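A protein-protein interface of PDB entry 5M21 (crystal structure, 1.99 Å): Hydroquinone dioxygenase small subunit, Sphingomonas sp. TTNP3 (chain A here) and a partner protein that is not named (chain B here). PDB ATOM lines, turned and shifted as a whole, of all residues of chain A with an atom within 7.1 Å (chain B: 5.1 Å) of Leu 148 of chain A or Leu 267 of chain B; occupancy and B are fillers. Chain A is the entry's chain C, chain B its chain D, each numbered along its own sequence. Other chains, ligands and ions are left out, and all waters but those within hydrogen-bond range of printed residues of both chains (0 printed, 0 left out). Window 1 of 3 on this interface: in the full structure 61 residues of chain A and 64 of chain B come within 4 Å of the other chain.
O of Ser 32 of chain A is in hydrogen-bond range of N of Ile 296 of chain B (3.0 Å).
The side-chain amide nitrogen (ND2) of Asn 33 of chain A lies within hydrogen-bond range of the side-chain carboxylate (OD1) of Asp 295 of chain B, 2.6 Å away.
The backbone carbonyl oxygen of Gly 294 of chain B lies within hydrogen-bond range of the backbone NH of Val 34 of chain A (2.8 Å).
N of Phe 35 of chain A is in hydrogen-bond range of OD1 of Asn 33 of chain A (2.9 Å).
The side-chain hydroxyl of Ser 59 of chain A is in hydrogen-bond range of the backbone carbonyl oxygen of Val 34 of chain A.
The backbone NH of Val 49 of chain A is in hydrogen-bond range of the backbone carbonyl oxygen of Ile 57 of chain A.
The backbone carbonyl oxygen (O) of Leu 78 of chain A sits at hydrogen-bond distance from the backbone NH (N) of Leu 148 of chain A (2.8 Å).
The backbone NH of Gly 294 of chain B sits at hydrogen-bond distance from the backbone carbonyl oxygen of Gln 268 of chain B, 2.9 Å away.
The backbone carbonyl oxygen (O) of Asp 295 of chain B sits at hydrogen-bond distance from the backbone NH (N) of Gln 268 of chain B.
Among the printed residues, merely in contact across the chains: Ser 32 of chain A with Gly 294 of chain B, Ser 32 of chain A with Asp 295 of chain B, Asn 33 of chain A with Gly 294 of chain B, Val 34 of chain A with Ile 296 of chain B, Phe 35 of chain A with Gly 294 of chain B, Val 49 of chain A with Trp 265 of chain B, Val 49 of chain A with Ile 296 of chain B and Leu 148 of chain A with Leu 267 of chain B.
Of chain B, only Leu 267 (3.5 Å) comes within 4 Å of Leu 148 of chain A.
Of the printed residues of chain B, Val 49 of chain A touches Trp 265 (3.4 Å) and Ile 296 (3.5 Å).
Of the printed residues of chain A, Ile 296 of chain B touches Ser 32 (3.0 Å), Val 34 (3.99 Å) and Val 49 (3.5 Å).
Of the printed residues of chain B, Phe 35 of chain A touches Gly 294 (3.7 Å).
Printed residues of chain A within 4 Å of Gly 294 of chain B: Ser 32, Asn 33, Val 34 and Phe 35.
Leu 269 of chain B touches none of the printed residues of chain A.
Gln 150 of chain A touches none of the printed residues of chain B.
The nearest residue of chain A that does not touch Leu 267 of chain B is Val 34 of chain A (4.1 Å).
The nearest printed residue of chain A that does not touch Trp 265 of chain B is Ile 57 of chain A (5.4 Å).
Of the 11 printed residues of chain B, 5 touch a printed residue of chain A.
Printed residues of chain B that touch a printed residue of chain A: Trp 265, Leu 267, Gly 294, Asp 295 and Ile 296.
Printed residues of chain A that touch a printed residue of chain B: Ser 32, Asn 33, Val 34, Phe 35, Val 49 and Leu 148.
Hydrophobic or aromatic side chains of chain A within 4 Å of the printed part of chain B: Val 34, Phe 35, Val 49 and Leu 148.
Along chain A the printed residues that touch a printed residue of chain B span positions 32 to 148.
Among the printed residues, 11 pairs touch across the chains.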
ATOM      1  N   SER A  32     -17.819  22.500   6.633  1.00  0.00           N
ATOM      2  CA  SER A  32     -17.251  23.808   6.879  1.00  0.00           C
ATOM      3  C   SER A  32     -17.179  24.520   5.530  1.00  0.00           C
ATOM      4  O   SER A  32     -17.424  23.910   4.513  1.00  0.00           O
ATOM      5  CB  SER A  32     -15.827  23.689   7.491  1.00  0.00           C
ATOM      6  OG  SER A  32     -14.880  23.274   6.479  1.00  0.00           O
ATOM      7  N   ASN A  33     -16.832  25.805   5.539  1.00  0.00           N
ATOM      8  CA  ASN A  33     -16.604  26.530   4.329  1.00  0.00           C
ATOM      9  C   ASN A  33     -15.152  26.972   4.335  1.00  0.00           C
ATOM     10  O   ASN A  33     -14.668  27.540   5.309  1.00  0.00           O
ATOM     11  CB  ASN A  33     -17.582  27.708   4.233  1.00  0.00           C
ATOM     12  CG  ASN A  33     -17.479  28.442   2.902  1.00  0.00           C
ATOM     13  OD1 ASN A  33     -16.510  29.199   2.683  1.00  0.00           O
ATOM     14  ND2 ASN A  33     -18.471  28.246   2.014  1.00  0.00           N
ATOM     15  N   VAL A  34     -14.437  26.685   3.255  1.00  0.00           N
ATOM     16  CA  VAL A  34     -13.002  26.966   3.198  1.00  0.00           C
ATOM     17  C   VAL A  34     -12.694  28.475   3.260  1.00  0.00           C
ATOM     18  O   VAL A  34     -11.623  28.867   3.659  1.00  0.00           O
ATOM     19  CB  VAL A  34     -12.313  26.302   1.964  1.00  0.00           C
ATOM     20  CG1 VAL A  34     -12.527  24.772   1.963  1.00  0.00           C
ATOM     21  CG2 VAL A  34     -12.776  26.942   0.637  1.00  0.00           C
ATOM     22  N   PHE A  35     -13.628  29.314   2.853  1.00  0.00           N
ATOM     23  CA  PHE A  35     -13.413  30.747   2.939  1.00  0.00           C
ATOM     24  C   PHE A  35     -13.548  31.250   4.338  1.00  0.00           C
ATOM     25  O   PHE A  35     -12.720  32.061   4.789  1.00  0.00           O
ATOM     26  CB  PHE A  35     -14.360  31.489   2.016  1.00  0.00           C
ATOM     27  CG  PHE A  35     -14.126  31.177   0.567  1.00  0.00           C
ATOM     28  CD1 PHE A  35     -12.992  31.672  -0.092  1.00  0.00           C
ATOM     29  CD2 PHE A  35     -15.021  30.367  -0.138  1.00  0.00           C
ATOM     30  CE1 PHE A  35     -12.770  31.400  -1.455  1.00  0.00           C
ATOM     31  CE2 PHE A  35     -14.787  30.069  -1.498  1.00  0.00           C
ATOM     32  CZ  PHE A  35     -13.687  30.578  -2.146  1.00  0.00           C
ATOM     33  N   VAL A  47      -4.954  25.041   7.907  1.00  0.00           N
ATOM     34  CA  VAL A  47      -6.017  24.431   8.710  1.00  0.00           C
ATOM     35  C   VAL A  47      -6.595  23.268   7.946  1.00  0.00           C
ATOM     36  O   VAL A  47      -7.025  23.453   6.785  1.00  0.00           O
ATOM     37  CB  VAL A  47      -7.128  25.479   9.006  1.00  0.00           C
ATOM     38  CG1 VAL A  47      -8.272  24.860   9.802  1.00  0.00           C
ATOM     39  CG2 VAL A  47      -6.534  26.622   9.797  1.00  0.00           C
ATOM     40  N   VAL A  49      -9.261  21.093   6.487  1.00  0.00           N
ATOM     41  CA  VAL A  49     -10.708  21.127   6.177  1.00  0.00           C
ATOM     42  C   VAL A  49     -11.285  19.815   5.622  1.00  0.00           C
ATOM     43  O   VAL A  49     -12.536  19.618   5.619  1.00  0.00           O
ATOM     44  CB  VAL A  49     -11.063  22.261   5.187  1.00  0.00           C
ATOM     45  CG1 VAL A  49     -10.822  23.614   5.801  1.00  0.00           C
ATOM     46  CG2 VAL A  49     -10.262  22.110   3.892  1.00  0.00           C
ATOM     47  N   ILE A  57      -6.876  18.022   3.097  1.00  0.00           N
ATOM     48  CA  ILE A  57      -6.991  19.226   2.331  1.00  0.00           C
ATOM     49  C   ILE A  57      -6.880  20.322   3.380  1.00  0.00           C
ATOM     50  O   ILE A  57      -7.505  20.245   4.439  1.00  0.00           O
ATOM     51  CB  ILE A  57      -8.311  19.314   1.534  1.00  0.00           C
ATOM     52  CG1 ILE A  57      -8.377  18.236   0.462  1.00  0.00           C
ATOM     53  CG2 ILE A  57      -8.427  20.690   0.861  1.00  0.00           C
ATOM     54  CD1 ILE A  57      -9.705  18.215  -0.302  1.00  0.00           C
ATOM     55  N   GLU A  58      -5.988  21.274   3.155  1.00  0.00           N
ATOM     56  CA  GLU A  58      -5.783  22.372   4.142  1.00  0.00           C
ATOM     57  C   GLU A  58      -6.256  23.686   3.535  1.00  0.00           C
ATOM     58  O   GLU A  58      -6.087  23.939   2.316  1.00  0.00           O
ATOM     59  CB  GLU A  58      -4.327  22.539   4.559  1.00  0.00           C
ATOM     60  CG  GLU A  58      -3.760  21.338   5.289  1.00  0.00           C
ATOM     61  CD  GLU A  58      -2.253  21.151   5.068  1.00  0.00           C
ATOM     62  OE1 GLU A  58      -1.640  21.575   3.997  1.00  0.00           O
ATOM     63  OE2 GLU A  58      -1.691  20.519   5.993  1.00  0.00           O
ATOM     64  N   SER A  59      -6.856  24.526   4.355  1.00  0.00           N
ATOM     65  CA  SER A  59      -7.260  25.829   3.812  1.00  0.00           C
ATOM     66  C   SER A  59      -6.335  26.865   4.380  1.00  0.00           C
ATOM     67  O   SER A  59      -6.113  26.849   5.581  1.00  0.00           O
ATOM     68  CB  SER A  59      -8.712  26.118   4.158  1.00  0.00           C
ATOM     69  OG  SER A  59      -9.044  27.491   3.860  1.00  0.00           O
ATOM     70  N   ALA A  60      -5.804  27.783   3.567  1.00  0.00           N
ATOM     71  CA  ALA A  60      -5.026  28.859   4.150  1.00  0.00           C
ATOM     72  C   ALA A  60      -5.302  30.231   3.541  1.00  0.00           C
ATOM     73  O   ALA A  60      -5.621  30.343   2.343  1.00  0.00           O
ATOM     74  CB  ALA A  60      -3.525  28.534   4.065  1.00  0.00           C
ATOM     75  N   PHE A  76      -0.051  19.912  -3.920  1.00  0.00           N
ATOM     76  CA  PHE A  76      -0.620  20.797  -4.925  1.00  0.00           C
ATOM     77  C   PHE A  76      -1.319  21.925  -4.201  1.00  0.00           C
ATOM     78  O   PHE A  76      -1.733  21.787  -3.054  1.00  0.00           O
ATOM     79  CB  PHE A  76      -1.570  20.079  -5.896  1.00  0.00           C
ATOM     80  CG  PHE A  76      -0.919  18.930  -6.627  1.00  0.00           C
ATOM     81  CD1 PHE A  76      -0.897  17.668  -6.047  1.00  0.00           C
ATOM     82  CD2 PHE A  76      -0.386  19.109  -7.896  1.00  0.00           C
ATOM     83  CE1 PHE A  76      -0.280  16.623  -6.704  1.00  0.00           C
ATOM     84  CE2 PHE A  76       0.222  18.067  -8.556  1.00  0.00           C
ATOM     85  CZ  PHE A  76       0.269  16.827  -7.961  1.00  0.00           C
ATOM     86  N   VAL A  77      -1.349  23.072  -4.850  1.00  0.00           N
ATOM     87  CA  VAL A  77      -1.989  24.248  -4.246  1.00  0.00           C
ATOM     88  C   VAL A  77      -2.973  24.760  -5.294  1.00  0.00           C
ATOM     89  O   VAL A  77      -2.636  24.903  -6.456  1.00  0.00           O
ATOM     90  CB  VAL A  77      -0.962  25.320  -3.826  1.00  0.00           C
ATOM     91  CG1 VAL A  77      -0.002  25.637  -4.962  1.00  0.00           C
ATOM     92  CG2 VAL A  77      -1.686  26.588  -3.344  1.00  0.00           C
ATOM     93  N   LEU A  78      -4.202  24.968  -4.846  1.00  0.00           N
ATOM     94  CA  LEU A  78      -5.238  25.544  -5.673  1.00  0.00           C
ATOM     95  C   LEU A  78      -5.598  26.914  -5.166  1.00  0.00           C
ATOM     96  O   LEU A  78      -6.001  27.066  -3.974  1.00  0.00           O
ATOM     97  CB  LEU A  78      -6.479  24.622  -5.710  1.00  0.00           C
ATOM     98  CG  LEU A  78      -7.752  25.192  -6.356  1.00  0.00           C
ATOM     99  CD1 LEU A  78      -7.595  25.411  -7.866  1.00  0.00           C
ATOM    100  CD2 LEU A  78      -8.880  24.222  -6.045  1.00  0.00           C
ATOM    101  N   ALA A  79      -5.435  27.925  -6.023  1.00  0.00           N
ATOM    102  CA  ALA A  79      -5.832  29.295  -5.603  1.00  0.00           C
ATOM    103  C   ALA A  79      -7.343  29.412  -5.671  1.00  0.00           C
ATOM    104  O   ALA A  79      -7.904  29.046  -6.680  1.00  0.00           O
ATOM    105  CB  ALA A  79      -5.147  30.375  -6.462  1.00  0.00           C
ATOM    106  N   MET A  80      -7.987  29.844  -4.575  1.00  0.00           N
ATOM    107  CA  MET A  80      -9.473  29.961  -4.520  1.00  0.00           C
ATOM    108  C   MET A  80     -10.034  31.383  -4.687  1.00  0.00           C
ATOM    109  O   MET A  80     -11.204  31.515  -5.080  1.00  0.00           O
ATOM    110  CB  MET A  80     -10.075  29.330  -3.247  1.00  0.00           C
ATOM    111  CG  MET A  80      -9.832  27.812  -3.180  1.00  0.00           C
ATOM    112  SD  MET A  80     -10.861  27.005  -4.419  1.00  0.00           S
ATOM    113  CE  MET A  80     -12.463  27.088  -3.599  1.00  0.00           C
ATOM    114  N   ILE A  84      -1.938  34.972  -6.040  1.00  0.00           N
ATOM    115  CA  ILE A  84      -0.911  34.437  -5.157  1.00  0.00           C
ATOM    116  C   ILE A  84       0.247  33.998  -6.015  1.00  0.00           C
ATOM    117  O   ILE A  84       0.084  33.184  -6.924  1.00  0.00           O
ATOM    118  CB  ILE A  84      -1.376  33.163  -4.370  1.00  0.00           C
ATOM    119  CG1 ILE A  84      -2.534  33.448  -3.407  1.00  0.00           C
ATOM    120  CG2 ILE A  84      -0.213  32.538  -3.599  1.00  0.00           C
ATOM    121  CD1 ILE A  84      -3.365  32.223  -3.025  1.00  0.00           C
ATOM    122  N   MET A 128      -4.329  25.936 -10.353  1.00  0.00           N
ATOM    123  CA  MET A 128      -3.682  24.940  -9.498  1.00  0.00           C
ATOM    124  C   MET A 128      -2.223  24.847  -9.897  1.00  0.00           C
ATOM    125  O   MET A 128      -1.897  24.829 -11.102  1.00  0.00           O
ATOM    126  CB  MET A 128      -4.360  23.549  -9.608  1.00  0.00           C
ATOM    127  CG  MET A 128      -3.421  22.434  -9.155  1.00  0.00           C
ATOM    128  SD  MET A 128      -4.112  20.758  -9.208  1.00  0.00           S
ATOM    129  CE  MET A 128      -5.224  20.889  -7.797  1.00  0.00           C
ATOM    130  N   LEU A 131       3.474  21.561  -6.483  1.00  0.00           N
ATOM    131  CA  LEU A 131       4.563  21.815  -5.551  1.00  0.00           C
ATOM    132  C   LEU A 131       5.406  20.536  -5.466  1.00  0.00           C
ATOM    133  O   LEU A 131       5.108  19.633  -4.648  1.00  0.00           O
ATOM    134  CB  LEU A 131       4.033  22.196  -4.161  1.00  0.00           C
ATOM    135  CG  LEU A 131       3.063  23.427  -4.147  1.00  0.00           C
ATOM    136  CD1 LEU A 131       2.449  23.477  -2.768  1.00  0.00           C
ATOM    137  CD2 LEU A 131       3.766  24.747  -4.441  1.00  0.00           C
ATOM    138  N   ALA A 146      -7.352  33.365  -0.730  1.00  0.00           N
ATOM    139  CA  ALA A 146      -7.668  32.027  -0.198  1.00  0.00           C
ATOM    140  C   ALA A 146      -6.962  30.960  -1.022  1.00  0.00           C
ATOM    141  O   ALA A 146      -6.870  31.074  -2.243  1.00  0.00           O
ATOM    142  CB  ALA A 146      -9.164  31.789  -0.183  1.00  0.00           C
ATOM    143  N   MET A 147      -6.396  29.958  -0.367  1.00  0.00           N
ATOM    144  CA  MET A 147      -5.775  28.847  -1.119  1.00  0.00           C
ATOM    145  C   MET A 147      -6.029  27.533  -0.462  1.00  0.00           C
ATOM    146  O   MET A 147      -6.293  27.475   0.743  1.00  0.00           O
ATOM    147  CB  MET A 147      -4.240  29.030  -1.350  1.00  0.00           C
ATOM    148  CG  MET A 147      -3.439  29.181  -0.079  1.00  0.00           C
ATOM    149  SD  MET A 147      -1.710  29.712  -0.341  1.00  0.00           S
ATOM    150  CE  MET A 147      -1.415  29.981   1.384  1.00  0.00           C
ATOM    151  N   LEU A 148      -5.887  26.462  -1.225  1.00  0.00           N
ATOM    152  CA  LEU A 148      -6.094  25.149  -0.642  1.00  0.00           C
ATOM    153  C   LEU A 148      -4.906  24.247  -0.977  1.00  0.00           C
ATOM    154  O   LEU A 148      -4.374  24.301  -2.092  1.00  0.00           O
ATOM    155  CB  LEU A 148      -7.360  24.487  -1.167  1.00  0.00           C
ATOM    156  CG  LEU A 148      -8.710  25.040  -0.750  1.00  0.00           C
ATOM    157  CD1 LEU A 148      -9.776  24.377  -1.605  1.00  0.00           C
ATOM    158  CD2 LEU A 148      -8.998  24.754   0.734  1.00  0.00           C
ATOM    159  N   PHE A 149      -4.521  23.408  -0.016  1.00  0.00           N
ATOM    160  CA  PHE A 149      -3.463  22.433  -0.285  1.00  0.00           C
ATOM    161  C   PHE A 149      -4.005  20.992  -0.342  1.00  0.00           C
ATOM    162  O   PHE A 149      -4.825  20.603   0.475  1.00  0.00           O
ATOM    163  CB  PHE A 149      -2.391  22.520   0.788  1.00  0.00           C
ATOM    164  CG  PHE A 149      -1.636  23.823   0.808  1.00  0.00           C
ATOM    165  CD1 PHE A 149      -0.459  23.971   0.067  1.00  0.00           C
ATOM    166  CD2 PHE A 149      -2.076  24.899   1.595  1.00  0.00           C
ATOM    167  CE1 PHE A 149       0.249  25.161   0.110  1.00  0.00           C
ATOM    168  CE2 PHE A 149      -1.372  26.098   1.622  1.00  0.00           C
ATOM    169  CZ  PHE A 149      -0.205  26.233   0.875  1.00  0.00           C
ATOM    170  N   GLN A 150      -3.529  20.240  -1.330  1.00  0.00           N
ATOM    171  CA  GLN A 150      -3.621  18.796  -1.356  1.00  0.00           C
ATOM    172  C   GLN A 150      -2.279  18.245  -0.762  1.00  0.00           C
ATOM    173  O   GLN A 150      -1.233  18.305  -1.437  1.00  0.00           O
ATOM    174  CB  GLN A 150      -3.802  18.295  -2.821  1.00  0.00           C
ATOM    175  CG  GLN A 150      -4.075  16.764  -2.947  1.00  0.00           C
ATOM    176  CD  GLN A 150      -4.208  16.304  -4.394  1.00  0.00           C
ATOM    177  OE1 GLN A 150      -4.143  17.100  -5.293  1.00  0.00           O
ATOM    178  NE2 GLN A 150      -4.442  15.014  -4.606  1.00  0.00           N
ATOM    179  N   TRP B 265     -14.898  13.001   0.173  1.00  0.00           N
ATOM    180  CA  TRP B 265     -15.143  14.399   0.464  1.00  0.00           C
ATOM    181  C   TRP B 265     -15.618  15.133  -0.777  1.00  0.00           C
ATOM    182  O   TRP B 265     -15.209  14.831  -1.883  1.00  0.00           O
ATOM    183  CB  TRP B 265     -13.918  15.053   1.053  1.00  0.00           C
ATOM    184  CG  TRP B 265     -13.585  14.589   2.441  1.00  0.00           C
ATOM    185  CD1 TRP B 265     -12.943  13.441   2.783  1.00  0.00           C
ATOM    186  CD2 TRP B 265     -13.828  15.290   3.661  1.00  0.00           C
ATOM    187  NE1 TRP B 265     -12.788  13.371   4.147  1.00  0.00           N
ATOM    188  CE2 TRP B 265     -13.293  14.509   4.708  1.00  0.00           C
ATOM    189  CE3 TRP B 265     -14.416  16.519   3.975  1.00  0.00           C
ATOM    190  CZ2 TRP B 265     -13.370  14.889   6.034  1.00  0.00           C
ATOM    191  CZ3 TRP B 265     -14.473  16.899   5.316  1.00  0.00           C
ATOM    192  CH2 TRP B 265     -13.961  16.095   6.313  1.00  0.00           C
ATOM    193  N   PHE B 266     -16.537  16.057  -0.561  1.00  0.00           N
ATOM    194  CA  PHE B 266     -17.027  16.892  -1.648  1.00  0.00           C
ATOM    195  C   PHE B 266     -16.618  18.326  -1.344  1.00  0.00           C
ATOM    196  O   PHE B 266     -16.916  18.806  -0.278  1.00  0.00           O
ATOM    197  CB  PHE B 266     -18.549  16.825  -1.680  1.00  0.00           C
ATOM    198  CG  PHE B 266     -19.119  15.520  -2.126  1.00  0.00           C
ATOM    199  CD1 PHE B 266     -18.433  14.681  -3.000  1.00  0.00           C
ATOM    200  CD2 PHE B 266     -20.452  15.179  -1.752  1.00  0.00           C
ATOM    201  CE1 PHE B 266     -19.020  13.502  -3.446  1.00  0.00           C
ATOM    202  CE2 PHE B 266     -21.027  14.005  -2.190  1.00  0.00           C
ATOM    203  CZ  PHE B 266     -20.302  13.179  -3.047  1.00  0.00           C
ATOM    204  N   LEU B 267     -15.937  18.991  -2.264  1.00  0.00           N
ATOM    205  CA  LEU B 267     -15.672  20.439  -2.154  1.00  0.00           C
ATOM    206  C   LEU B 267     -16.367  21.186  -3.313  1.00  0.00           C
ATOM    207  O   LEU B 267     -16.030  20.970  -4.491  1.00  0.00           O
ATOM    208  CB  LEU B 267     -14.177  20.754  -2.169  1.00  0.00           C
ATOM    209  CG  LEU B 267     -13.795  22.233  -2.516  1.00  0.00           C
ATOM    210  CD1 LEU B 267     -14.185  23.211  -1.433  1.00  0.00           C
ATOM    211  CD2 LEU B 267     -12.337  22.382  -2.813  1.00  0.00           C
ATOM    212  N   GLN B 268     -17.363  22.012  -2.979  1.00  0.00           N
ATOM    213  CA  GLN B 268     -18.166  22.693  -4.023  1.00  0.00           C
ATOM    214  C   GLN B 268     -17.384  23.854  -4.575  1.00  0.00           C
ATOM    215  O   GLN B 268     -16.967  24.705  -3.806  1.00  0.00           O
ATOM    216  CB  GLN B 268     -19.483  23.204  -3.427  1.00  0.00           C
ATOM    217  CG  GLN B 268     -20.480  23.731  -4.471  1.00  0.00           C
ATOM    218  CD  GLN B 268     -20.976  22.624  -5.343  1.00  0.00           C
ATOM    219  OE1 GLN B 268     -21.199  21.521  -4.831  1.00  0.00           O
ATOM    220  NE2 GLN B 268     -21.110  22.870  -6.672  1.00  0.00           N
ATOM    221  N   LEU B 269     -17.129  23.902  -5.874  1.00  0.00           N
ATOM    222  CA  LEU B 269     -16.271  24.994  -6.394  1.00  0.00           C
ATOM    223  C   LEU B 269     -17.038  26.203  -6.964  1.00  0.00           C
ATOM    224  O   LEU B 269     -16.523  27.356  -7.031  1.00  0.00           O
ATOM    225  CB  LEU B 269     -15.232  24.484  -7.398  1.00  0.00           C
ATOM    226  CG  LEU B 269     -14.302  23.364  -6.923  1.00  0.00           C
ATOM    227  CD1 LEU B 269     -13.721  22.637  -8.154  1.00  0.00           C
ATOM    228  CD2 LEU B 269     -13.213  23.894  -5.961  1.00  0.00           C
ATOM    229  N   GLY B 294     -17.271  26.871  -1.964  1.00  0.00           N
ATOM    230  CA  GLY B 294     -16.328  26.750  -0.834  1.00  0.00           C
ATOM    231  C   GLY B 294     -16.777  25.794   0.266  1.00  0.00           C
ATOM    232  O   GLY B 294     -15.982  25.548   1.179  1.00  0.00           O
ATOM    233  N   ASP B 295     -18.037  25.306   0.233  1.00  0.00           N
ATOM    234  CA  ASP B 295     -18.468  24.297   1.203  1.00  0.00           C
ATOM    235  C   ASP B 295     -17.769  22.950   0.891  1.00  0.00           C
ATOM    236  O   ASP B 295     -17.694  22.505  -0.279  1.00  0.00           O
ATOM    237  CB  ASP B 295     -19.997  24.096   1.313  1.00  0.00           C
ATOM    238  CG  ASP B 295     -20.777  25.379   1.674  1.00  0.00           C
ATOM    239  OD1 ASP B 295     -20.213  26.303   2.319  1.00  0.00           O
ATOM    240  OD2 ASP B 295     -21.970  25.473   1.297  1.00  0.00           O
ATOM    241  N   ILE B 296     -17.223  22.344   1.950  1.00  0.00           N
ATOM    242  CA  ILE B 296     -16.555  21.050   1.901  1.00  0.00           C
ATOM    243  C   ILE B 296     -17.191  20.214   3.004  1.00  0.00           C
ATOM    244  O   ILE B 296     -17.429  20.699   4.116  1.00  0.00           O
ATOM    245  CB  ILE B 296     -15.042  21.140   2.113  1.00  0.00           C
ATOM    246  CG1 ILE B 296     -14.379  19.747   2.044  1.00  0.00           C
ATOM    247  CG2 ILE B 296     -14.694  21.774   3.454  1.00  0.00           C
ATOM    248  CD1 ILE B 296     -12.866  19.807   2.125  1.00  0.00           C
ATOM    249  N   MET B 314     -19.253  23.294 -10.735  1.00  0.00           N
ATOM    250  CA  MET B 314     -17.966  22.691 -10.566  1.00  0.00           C
ATOM    251  C   MET B 314     -17.878  22.107  -9.163  1.00  0.00           C
ATOM    252  O   MET B 314     -18.118  22.814  -8.181  1.00  0.00           O
ATOM    253  CB  MET B 314     -16.916  23.783 -10.736  1.00  0.00           C
ATOM    254  CG  MET B 314     -16.807  24.279 -12.155  1.00  0.00           C
ATOM    255  SD  MET B 314     -15.593  25.588 -12.225  1.00  0.00           S
ATOM    256  CE  MET B 314     -15.899  26.070 -13.931  1.00  0.00           C
ATOM    257  N   LEU B 315     -17.568  20.809  -9.094  1.00  0.00           N
ATOM    258  CA  LEU B 315     -17.407  20.055  -7.855  1.00  0.00           C
ATOM    259  C   LEU B 315     -16.040  19.366  -7.874  1.00  0.00           C
ATOM    260  O   LEU B 315     -15.641  18.766  -8.882  1.00  0.00           O
ATOM    261  CB  LEU B 315     -18.503  18.967  -7.744  1.00  0.00           C
ATOM    262  CG  LEU B 315     -18.417  17.966  -6.569  1.00  0.00           C
ATOM    263  CD1 LEU B 315     -18.582  18.678  -5.230  1.00  0.00           C
ATOM    264  CD2 LEU B 315     -19.450  16.830  -6.746  1.00  0.00           C
ATOM    265  N   LEU B 316     -15.325  19.450  -6.765  1.00  0.00           N
ATOM    266  CA  LEU B 316     -14.205  18.554  -6.533  1.00  0.00           C
ATOM    267  C   LEU B 316     -14.646  17.303  -5.764  1.00  0.00           C
ATOM    268  O   LEU B 316     -15.071  17.422  -4.626  1.00  0.00           O
ATOM    269  CB  LEU B 316     -13.158  19.266  -5.679  1.00  0.00           C
ATOM    270  CG  LEU B 316     -11.944  18.426  -5.196  1.00  0.00           C
ATOM    271  CD1 LEU B 316     -11.089  17.963  -6.363  1.00  0.00           C
ATOM    272  CD2 LEU B 316     -11.066  19.258  -4.259  1.00  0.00           C
